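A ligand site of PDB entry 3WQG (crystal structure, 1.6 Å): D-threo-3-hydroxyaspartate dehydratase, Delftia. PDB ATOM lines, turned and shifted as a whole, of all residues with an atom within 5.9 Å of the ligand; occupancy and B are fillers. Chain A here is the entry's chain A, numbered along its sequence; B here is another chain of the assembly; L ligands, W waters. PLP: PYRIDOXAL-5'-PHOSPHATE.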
ATOM      1  N   HIS A  51      19.277   9.166 -21.186  1.00  0.00           N
ATOM      2  CA  HIS A  51      18.010   8.626 -21.478  1.00  0.00           C
ATOM      3  C   HIS A  51      16.957   9.282 -20.588  1.00  0.00           C
ATOM      4  O   HIS A  51      17.007   9.124 -19.336  1.00  0.00           O
ATOM      5  CB  HIS A  51      18.002   7.121 -21.252  1.00  0.00           C
ATOM      6  CG  HIS A  51      16.881   6.429 -22.011  1.00  0.00           C
ATOM      7  ND1 HIS A  51      15.606   6.971 -22.082  1.00  0.00           N
ATOM      8  CD2 HIS A  51      16.921   5.384 -22.892  1.00  0.00           C
ATOM      9  CE1 HIS A  51      14.853   6.244 -22.933  1.00  0.00           C
ATOM     10  NE2 HIS A  51      15.652   5.243 -23.433  1.00  0.00           N
ATOM     11  N   LYS A  53      13.840   8.762 -20.243  1.00  0.00           N
ATOM     12  CA  LYS A  53      12.649   8.029 -19.771  1.00  0.00           C
ATOM     13  C   LYS A  53      12.606   7.993 -18.233  1.00  0.00           C
ATOM     14  O   LYS A  53      11.532   7.702 -17.689  1.00  0.00           O
ATOM     15  CB  LYS A  53      12.617   6.620 -20.374  1.00  0.00           C
ATOM     16  CG  LYS A  53      13.598   5.625 -19.735  1.00  0.00           C
ATOM     17  CD  LYS A  53      13.381   4.271 -20.369  1.00  0.00           C
ATOM     18  CE  LYS A  53      14.275   3.171 -19.726  1.00  0.00           C
ATOM     19  NZ  LYS A  53      15.308   2.624 -20.597  1.00  0.00           N
ATOM     20  N   THR A  54      13.711   8.226 -17.537  1.00  0.00           N
ATOM     21  CA  THR A  54      13.715   8.251 -16.041  1.00  0.00           C
ATOM     22  C   THR A  54      12.872   9.401 -15.520  1.00  0.00           C
ATOM     23  O   THR A  54      12.121   9.204 -14.511  1.00  0.00           O
ATOM     24  CB  THR A  54      15.143   8.316 -15.541  1.00  0.00           C
ATOM     25  OG1 THR A  54      15.864   7.203 -16.063  1.00  0.00           O
ATOM     26  CG2 THR A  54      15.162   8.310 -13.987  1.00  0.00           C
ATOM     27  N   THR A  73      18.067  10.293 -25.489  1.00  0.00           N
ATOM     28  CA  THR A  73      17.374   9.037 -25.846  1.00  0.00           C
ATOM     29  C   THR A  73      16.009   9.111 -25.245  1.00  0.00           C
ATOM     30  O   THR A  73      15.888   9.609 -24.109  1.00  0.00           O
ATOM     31  CB  THR A  73      18.123   7.822 -25.251  1.00  0.00           C
ATOM     32  OG1 THR A  73      19.555   7.902 -25.514  1.00  0.00           O
ATOM     33  CG2 THR A  73      17.617   6.526 -25.967  1.00  0.00           C
ATOM     34  N   ALA A  94      14.712   4.884 -28.788  1.00  0.00           N
ATOM     35  CA  ALA A  94      15.448   3.604 -28.588  1.00  0.00           C
ATOM     36  C   ALA A  94      14.446   2.465 -28.191  1.00  0.00           C
ATOM     37  O   ALA A  94      14.737   1.741 -27.227  1.00  0.00           O
ATOM     38  CB  ALA A  94      16.591   3.746 -27.589  1.00  0.00           C
ATOM     39  N   ILE A 118      15.215   2.858 -34.452  1.00  0.00           N
ATOM     40  CA  ILE A 118      16.004   1.634 -34.345  1.00  0.00           C
ATOM     41  C   ILE A 118      15.134   0.473 -34.841  1.00  0.00           C
ATOM     42  O   ILE A 118      13.884   0.422 -34.703  1.00  0.00           O
ATOM     43  CB  ILE A 118      16.557   1.390 -32.888  1.00  0.00           C
ATOM     44  CG1 ILE A 118      15.450   0.891 -31.893  1.00  0.00           C
ATOM     45  CG2 ILE A 118      17.170   2.706 -32.400  1.00  0.00           C
ATOM     46  CD1 ILE A 118      16.116   0.523 -30.525  1.00  0.00           C
ATOM     47  N   GLU A 144      19.654  -2.423 -33.752  1.00  0.00           N
ATOM     48  CA  GLU A 144      19.855  -2.791 -32.298  1.00  0.00           C
ATOM     49  C   GLU A 144      20.519  -4.190 -32.238  1.00  0.00           C
ATOM     50  O   GLU A 144      20.023  -5.123 -32.914  1.00  0.00           O
ATOM     51  CB  GLU A 144      18.504  -2.809 -31.568  1.00  0.00           C
ATOM     52  CG  GLU A 144      18.683  -3.025 -30.096  1.00  0.00           C
ATOM     53  CD  GLU A 144      17.412  -2.849 -29.264  1.00  0.00           C
ATOM     54  OE1 GLU A 144      17.642  -2.775 -27.992  1.00  0.00           O
ATOM     55  OE2 GLU A 144      16.283  -2.890 -29.799  1.00  0.00           O
ATOM     56  N   ARG A 151      16.751  -8.569 -24.062  1.00  0.00           N
ATOM     57  CA  ARG A 151      15.502  -7.971 -24.611  1.00  0.00           C
ATOM     58  C   ARG A 151      15.554  -8.039 -26.173  1.00  0.00           C
ATOM     59  O   ARG A 151      15.701  -9.150 -26.753  1.00  0.00           O
ATOM     60  CB  ARG A 151      15.390  -6.491 -24.115  1.00  0.00           C
ATOM     61  CG  ARG A 151      13.961  -5.943 -24.192  1.00  0.00           C
ATOM     62  CD  ARG A 151      13.859  -4.714 -23.306  1.00  0.00           C
ATOM     63  NE  ARG A 151      14.638  -3.585 -23.864  1.00  0.00           N
ATOM     64  CZ  ARG A 151      14.963  -2.510 -23.137  1.00  0.00           C
ATOM     65  NH1 ARG A 151      14.743  -2.541 -21.780  1.00  0.00           N
ATOM     66  NH2 ARG A 151      15.598  -1.455 -23.753  1.00  0.00           N
ATOM     67  N   LEU A 180      23.352   0.079 -31.898  1.00  0.00           N
ATOM     68  CA  LEU A 180      23.309   0.350 -30.442  1.00  0.00           C
ATOM     69  C   LEU A 180      23.039  -0.961 -29.739  1.00  0.00           C
ATOM     70  O   LEU A 180      22.418  -1.842 -30.311  1.00  0.00           O
ATOM     71  CB  LEU A 180      22.220   1.374 -30.059  1.00  0.00           C
ATOM     72  CG  LEU A 180      20.744   0.924 -30.081  1.00  0.00           C
ATOM     73  CD1 LEU A 180      19.881   1.972 -29.342  1.00  0.00           C
ATOM     74  CD2 LEU A 180      20.217   0.777 -31.525  1.00  0.00           C
ATOM     75  N   THR A 181      23.401  -0.970 -28.450  1.00  0.00           N
ATOM     76  CA  THR A 181      22.998  -2.108 -27.601  1.00  0.00           C
ATOM     77  C   THR A 181      22.736  -1.584 -26.207  1.00  0.00           C
ATOM     78  O   THR A 181      23.350  -0.525 -25.806  1.00  0.00           O
ATOM     79  CB  THR A 181      24.110  -3.203 -27.581  1.00  0.00           C
ATOM     80  OG1 THR A 181      23.579  -4.374 -26.928  1.00  0.00           O
ATOM     81  CG2 THR A 181      25.337  -2.681 -26.880  1.00  0.00           C
ATOM     82  N   HIS A 182      21.928  -2.330 -25.463  1.00  0.00           N
ATOM     83  CA  HIS A 182      21.646  -1.981 -24.063  1.00  0.00           C
ATOM     84  C   HIS A 182      21.803  -3.264 -23.280  1.00  0.00           C
ATOM     85  O   HIS A 182      20.944  -4.172 -23.430  1.00  0.00           O
ATOM     86  CB  HIS A 182      20.193  -1.454 -24.000  1.00  0.00           C
ATOM     87  CG  HIS A 182      19.639  -1.283 -22.592  1.00  0.00           C
ATOM     88  ND1 HIS A 182      20.153  -0.416 -21.683  1.00  0.00           N
ATOM     89  CD2 HIS A 182      18.530  -1.927 -21.980  1.00  0.00           C
ATOM     90  CE1 HIS A 182      19.365  -0.479 -20.514  1.00  0.00           C
ATOM     91  NE2 HIS A 182      18.368  -1.376 -20.730  1.00  0.00           N
ATOM     92  N   SER A 186      22.481  -6.108 -16.692  1.00  0.00           N
ATOM     93  CA  SER A 186      23.339  -5.538 -15.616  1.00  0.00           C
ATOM     94  C   SER A 186      22.509  -5.360 -14.318  1.00  0.00           C
ATOM     95  O   SER A 186      23.089  -5.412 -13.198  1.00  0.00           O
ATOM     96  CB  SER A 186      23.990  -4.215 -16.032  1.00  0.00           C
ATOM     97  OG  SER A 186      22.952  -3.225 -16.184  1.00  0.00           O
ATOM     98  N   TYR A 187      21.212  -5.248 -14.461  1.00  0.00           N
ATOM     99  CA  TYR A 187      20.346  -5.030 -13.274  1.00  0.00           C
ATOM    100  C   TYR A 187      20.308  -6.245 -12.386  1.00  0.00           C
ATOM    101  O   TYR A 187      19.959  -6.151 -11.177  1.00  0.00           O
ATOM    102  CB  TYR A 187      18.918  -4.635 -13.730  1.00  0.00           C
ATOM    103  CG  TYR A 187      18.821  -3.157 -14.055  1.00  0.00           C
ATOM    104  CD1 TYR A 187      19.622  -2.570 -15.036  1.00  0.00           C
ATOM    105  CD2 TYR A 187      17.908  -2.324 -13.312  1.00  0.00           C
ATOM    106  CE1 TYR A 187      19.534  -1.218 -15.324  1.00  0.00           C
ATOM    107  CE2 TYR A 187      17.842  -0.934 -13.568  1.00  0.00           C
ATOM    108  CZ  TYR A 187      18.659  -0.417 -14.602  1.00  0.00           C
ATOM    109  OH  TYR A 187      18.628   0.927 -14.922  1.00  0.00           O
ATOM    110  N   GLY A 226      24.998   1.050 -23.541  1.00  0.00           N
ATOM    111  CA  GLY A 226      24.915   1.537 -22.156  1.00  0.00           C
ATOM    112  C   GLY A 226      23.698   1.101 -21.375  1.00  0.00           C
ATOM    113  O   GLY A 226      22.630   0.908 -21.946  1.00  0.00           O
ATOM    114  N   SER A 227      23.904   1.034 -20.086  1.00  0.00           N
ATOM    115  CA  SER A 227      22.872   1.015 -19.067  1.00  0.00           C
ATOM    116  C   SER A 227      23.583   1.793 -17.949  1.00  0.00           C
ATOM    117  O   SER A 227      24.798   1.974 -18.001  1.00  0.00           O
ATOM    118  CB  SER A 227      22.487  -0.451 -18.611  1.00  0.00           C
ATOM    119  OG  SER A 227      23.644  -1.068 -18.026  1.00  0.00           O
ATOM    120  N   THR A 228      22.871   2.268 -16.935  1.00  0.00           N
ATOM    121  CA  THR A 228      23.608   3.021 -15.877  1.00  0.00           C
ATOM    122  C   THR A 228      24.710   2.127 -15.240  1.00  0.00           C
ATOM    123  O   THR A 228      25.807   2.648 -15.019  1.00  0.00           O
ATOM    124  CB  THR A 228      22.615   3.578 -14.784  1.00  0.00           C
ATOM    125  OG1 THR A 228      22.074   4.803 -15.390  1.00  0.00           O
ATOM    126  CG2 THR A 228      23.351   4.005 -13.542  1.00  0.00           C
ATOM    127  N   PRO A 229      24.393   0.854 -14.897  1.00  0.00           N
ATOM    128  CA  PRO A 229      25.477   0.097 -14.170  1.00  0.00           C
ATOM    129  C   PRO A 229      26.703  -0.178 -15.071  1.00  0.00           C
ATOM    130  O   PRO A 229      27.847  -0.066 -14.592  1.00  0.00           O
ATOM    131  CB  PRO A 229      24.776  -1.264 -13.798  1.00  0.00           C
ATOM    132  CG  PRO A 229      23.308  -0.829 -13.617  1.00  0.00           C
ATOM    133  CD  PRO A 229      23.085   0.165 -14.813  1.00  0.00           C
ATOM    134  N   ARG A 244      24.642   5.593 -23.422  1.00  0.00           N
ATOM    135  CA  ARG A 244      23.283   6.008 -22.995  1.00  0.00           C
ATOM    136  C   ARG A 244      23.078   5.555 -21.555  1.00  0.00           C
ATOM    137  O   ARG A 244      23.254   4.348 -21.248  1.00  0.00           O
ATOM    138  CB  ARG A 244      22.198   5.388 -23.881  1.00  0.00           C
ATOM    139  CG  ARG A 244      22.489   5.626 -25.375  1.00  0.00           C
ATOM    140  CD  ARG A 244      21.370   5.058 -26.276  1.00  0.00           C
ATOM    141  NE  ARG A 244      21.002   3.720 -25.836  1.00  0.00           N
ATOM    142  CZ  ARG A 244      21.829   2.631 -25.894  1.00  0.00           C
ATOM    143  NH1 ARG A 244      22.920   2.600 -26.690  1.00  0.00           N
ATOM    144  NH2 ARG A 244      21.444   1.514 -25.276  1.00  0.00           N
ATOM    145  N   ALA A 245      22.649   6.513 -20.702  1.00  0.00           N
ATOM    146  CA  ALA A 245      22.340   6.141 -19.334  1.00  0.00           C
ATOM    147  C   ALA A 245      21.239   7.103 -18.874  1.00  0.00           C
ATOM    148  O   ALA A 245      21.243   8.266 -19.298  1.00  0.00           O
ATOM    149  CB  ALA A 245      23.527   6.295 -18.420  1.00  0.00           C
ATOM    150  N   GLY A 246      20.390   6.656 -17.959  1.00  0.00           N
ATOM    151  CA  GLY A 246      19.256   7.553 -17.539  1.00  0.00           C
ATOM    152  C   GLY A 246      18.999   7.500 -16.035  1.00  0.00           C
ATOM    153  O   GLY A 246      18.850   8.564 -15.434  1.00  0.00           O
ATOM    154  N   VAL A 247      18.977   6.288 -15.429  1.00  0.00           N
ATOM    155  CA  VAL A 247      18.488   6.233 -14.025  1.00  0.00           C
ATOM    156  C   VAL A 247      19.482   6.947 -13.123  1.00  0.00           C
ATOM    157  O   VAL A 247      19.099   7.462 -12.048  1.00  0.00           O
ATOM    158  CB  VAL A 247      18.172   4.776 -13.590  1.00  0.00           C
ATOM    159  CG1 VAL A 247      19.425   3.951 -13.353  1.00  0.00           C
ATOM    160  CG2 VAL A 247      17.282   4.865 -12.323  1.00  0.00           C
ATOM    161  N   TYR A 248      20.754   6.999 -13.517  1.00  0.00           N
ATOM    162  CA  TYR A 248      21.802   7.606 -12.676  1.00  0.00           C
ATOM    163  C   TYR A 248      21.470   9.069 -12.271  1.00  0.00           C
ATOM    164  O   TYR A 248      22.007   9.576 -11.292  1.00  0.00           O
ATOM    165  CB  TYR A 248      23.133   7.633 -13.494  1.00  0.00           C
ATOM    166  CG  TYR A 248      23.128   8.796 -14.473  1.00  0.00           C
ATOM    167  CD1 TYR A 248      22.574   8.663 -15.766  1.00  0.00           C
ATOM    168  CD2 TYR A 248      23.724  10.050 -14.119  1.00  0.00           C
ATOM    169  CE1 TYR A 248      22.496   9.773 -16.661  1.00  0.00           C
ATOM    170  CE2 TYR A 248      23.697  11.159 -14.960  1.00  0.00           C
ATOM    171  CZ  TYR A 248      23.046  11.008 -16.242  1.00  0.00           C
ATOM    172  OH  TYR A 248      23.041  12.087 -17.089  1.00  0.00           O
ATOM    173  N   MET A 255      19.699   0.495  -7.666  1.00  0.00           N
ATOM    174  CA  MET A 255      21.101   0.873  -8.051  1.00  0.00           C
ATOM    175  C   MET A 255      22.073   0.753  -6.884  1.00  0.00           C
ATOM    176  O   MET A 255      23.217   0.277  -7.035  1.00  0.00           O
ATOM    177  CB  MET A 255      21.172   2.294  -8.650  1.00  0.00           C
ATOM    178  CG  MET A 255      20.365   2.395  -9.980  1.00  0.00           C
ATOM    179  SD  MET A 255      21.392   1.492 -11.279  1.00  0.00           S
ATOM    180  CE  MET A 255      19.924   0.650 -11.591  1.00  0.00           C
ATOM    181  N   GLN B 329      10.486  -1.153 -19.261  1.00  0.00           N
ATOM    182  CA  GLN B 329       9.666   0.033 -19.149  1.00  0.00           C
ATOM    183  C   GLN B 329       8.626   0.144 -20.296  1.00  0.00           C
ATOM    184  O   GLN B 329       7.408   0.338 -20.100  1.00  0.00           O
ATOM    185  CB  GLN B 329      10.544   1.272 -19.024  1.00  0.00           C
ATOM    186  CG  GLN B 329       9.765   2.510 -18.633  1.00  0.00           C
ATOM    187  CD  GLN B 329      10.688   3.608 -18.101  1.00  0.00           C
ATOM    188  OE1 GLN B 329      11.700   3.355 -17.435  1.00  0.00           O
ATOM    189  NE2 GLN B 329      10.269   4.866 -18.383  1.00  0.00           N
ATOM    190  N   HIS B 331       8.747  -2.144 -23.115  1.00  0.00           N
ATOM    191  CA  HIS B 331       8.730  -3.412 -23.849  1.00  0.00           C
ATOM    192  C   HIS B 331       8.137  -4.447 -22.957  1.00  0.00           C
ATOM    193  O   HIS B 331       8.641  -4.650 -21.816  1.00  0.00           O
ATOM    194  CB  HIS B 331      10.174  -3.964 -24.041  1.00  0.00           C
ATOM    195  CG  HIS B 331      11.118  -3.084 -24.801  1.00  0.00           C
ATOM    196  ND1 HIS B 331      11.674  -1.922 -24.284  1.00  0.00           N
ATOM    197  CD2 HIS B 331      11.644  -3.241 -26.058  1.00  0.00           C
ATOM    198  CE1 HIS B 331      12.535  -1.385 -25.196  1.00  0.00           C
ATOM    199  NE2 HIS B 331      12.529  -2.200 -26.287  1.00  0.00           N
HETATM  200  N1  PLP L   1      19.380   2.300 -23.454  1.00  0.00           N
HETATM  201  C2  PLP L   1      18.142   1.827 -23.664  1.00  0.00           C
HETATM  202  C2A PLP L   1      17.695   1.112 -24.929  1.00  0.00           C
HETATM  203  C3  PLP L   1      17.172   1.923 -22.574  1.00  0.00           C
HETATM  204  O3  PLP L   1      15.963   1.483 -22.770  1.00  0.00           O
HETATM  205  C4  PLP L   1      17.557   2.615 -21.370  1.00  0.00           C
HETATM  206  C4A PLP L   1      16.552   2.890 -20.363  1.00  0.00           C
HETATM  207  C5  PLP L   1      18.946   3.095 -21.236  1.00  0.00           C
HETATM  208  C6  PLP L   1      19.801   2.902 -22.345  1.00  0.00           C
HETATM  209  C5A PLP L   1      19.462   3.819 -19.991  1.00  0.00           C
HETATM  210  O4P PLP L   1      19.721   2.728 -19.065  1.00  0.00           O
HETATM  211  P   PLP L   1      19.424   2.896 -17.491  1.00  0.00           P
HETATM  212  O1P PLP L   1      20.105   4.136 -17.112  1.00  0.00           O
HETATM  213  O2P PLP L   1      20.145   1.735 -16.788  1.00  0.00           O
HETATM  214  O3P PLP L   1      17.940   2.967 -17.475  1.00  0.00           O
HETATM  215  O   HOH W   1      15.596  -0.993 -26.710  1.00  0.00           O
HETATM  216  O   HOH W   2      14.332   3.138 -24.638  1.00  0.00           O
HETATM  217  O   HOH W   3      17.032   5.434 -18.195  1.00  0.00           O
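The guanidinium group (NH2) of Arg 151 sits at hydrogen-bond distance from an oxygen (O3) of the ligand, at 3.1 Å.
The guanidinium group (NH2) of Arg 244 sits at hydrogen-bond distance from a nitrogen (N1) of the ligand, at 2.9 Å.
The backbone NH (N) of Thr 228 lies within hydrogen-bond range of an oxygen (O2P) of the ligand (2.8 Å).
OG1 of Thr 228 sits at hydrogen-bond distance from O1P of the ligand, at 2.7 Å.
A nitrogen (N1) of the ligand sits at hydrogen-bond distance from a ring nitrogen (ND1) of His 182 (3.3 Å).
An oxygen (O1P) of the ligand is in hydrogen-bond range of the backbone NH (N) of Gly 246.
O1P of the ligand sits at hydrogen-bond distance from N of Val 247 (3.0 Å).
The side-chain hydroxyl (OH) of Tyr 187 is in hydrogen-bond range of an oxygen (O2P) of the ligand, at 2.5 Å.
A carbon (C4A) of the ligand is bonded to the side-chain amino group of Lys 53, at 1.3 Å.
OG1 of Thr 54 lies close to O of Gly 246 (3.3 Å).
The backbone NH of Lys 53 is in hydrogen-bond range of a ring nitrogen (ND1) of His 51 (3.1 Å).
O of Lys 53 is in hydrogen-bond range of NE2 of Gln 329 of chain B, at 3.2 Å.
The backbone NH of His 51 lies within hydrogen-bond range of the backbone carbonyl oxygen of Ala 245, 2.9 Å away.
OG1 of Thr 228 lies within hydrogen-bond range of N of Tyr 248, 3.2 Å away.
ND1 of His 51 is in hydrogen-bond range of O of Thr 73 (3.3 Å).
The side-chain hydroxyl of Thr 54 lies within hydrogen-bond range of the backbone NH of Val 247.
A ring nitrogen (ND1) of His 331 of chain B sits close to the guanidinium group of Arg 151 (3.4 Å).
Residues that only touch the ligand: His 51, Gly 226, Ser 227, Ala 245, Ala 94 and Pro 229.
Hydrophobic or aromatic side chains that line the ligand: His 51, Ala 94, His 182, Tyr 187, Pro 229 and Val 247.
Along chain A the residues within 4 Å of the ligand span positions 51 to 247.
The nearest printed residue that does not touch the ligand is Tyr 248 (4.6 Å).
Water W3 lies within hydrogen-bond range of an oxygen (O3P) of the ligand (2.7 Å), the side-chain hydroxyl (OG1) of Thr 54 (3.0 Å) and the backbone NH (N) of Val 247 (3.5 Å).
Water W2 lies within hydrogen-bond range of a ring nitrogen (NE2) of His 51, the backbone carbonyl oxygen of Ala 94 and an oxygen (O3) of the ligand.
Water W1 lies within hydrogen-bond range of the backbone carbonyl oxygen (O) of Ala 94 (2.9 Å), the guanidinium group (NH2) of Arg 151 (3.0 Å), the side-chain carboxylate (OE1) of Glu 144 (3.0 Å) and a ring nitrogen (NE2) of His 331 of chain B (3.3 Å).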
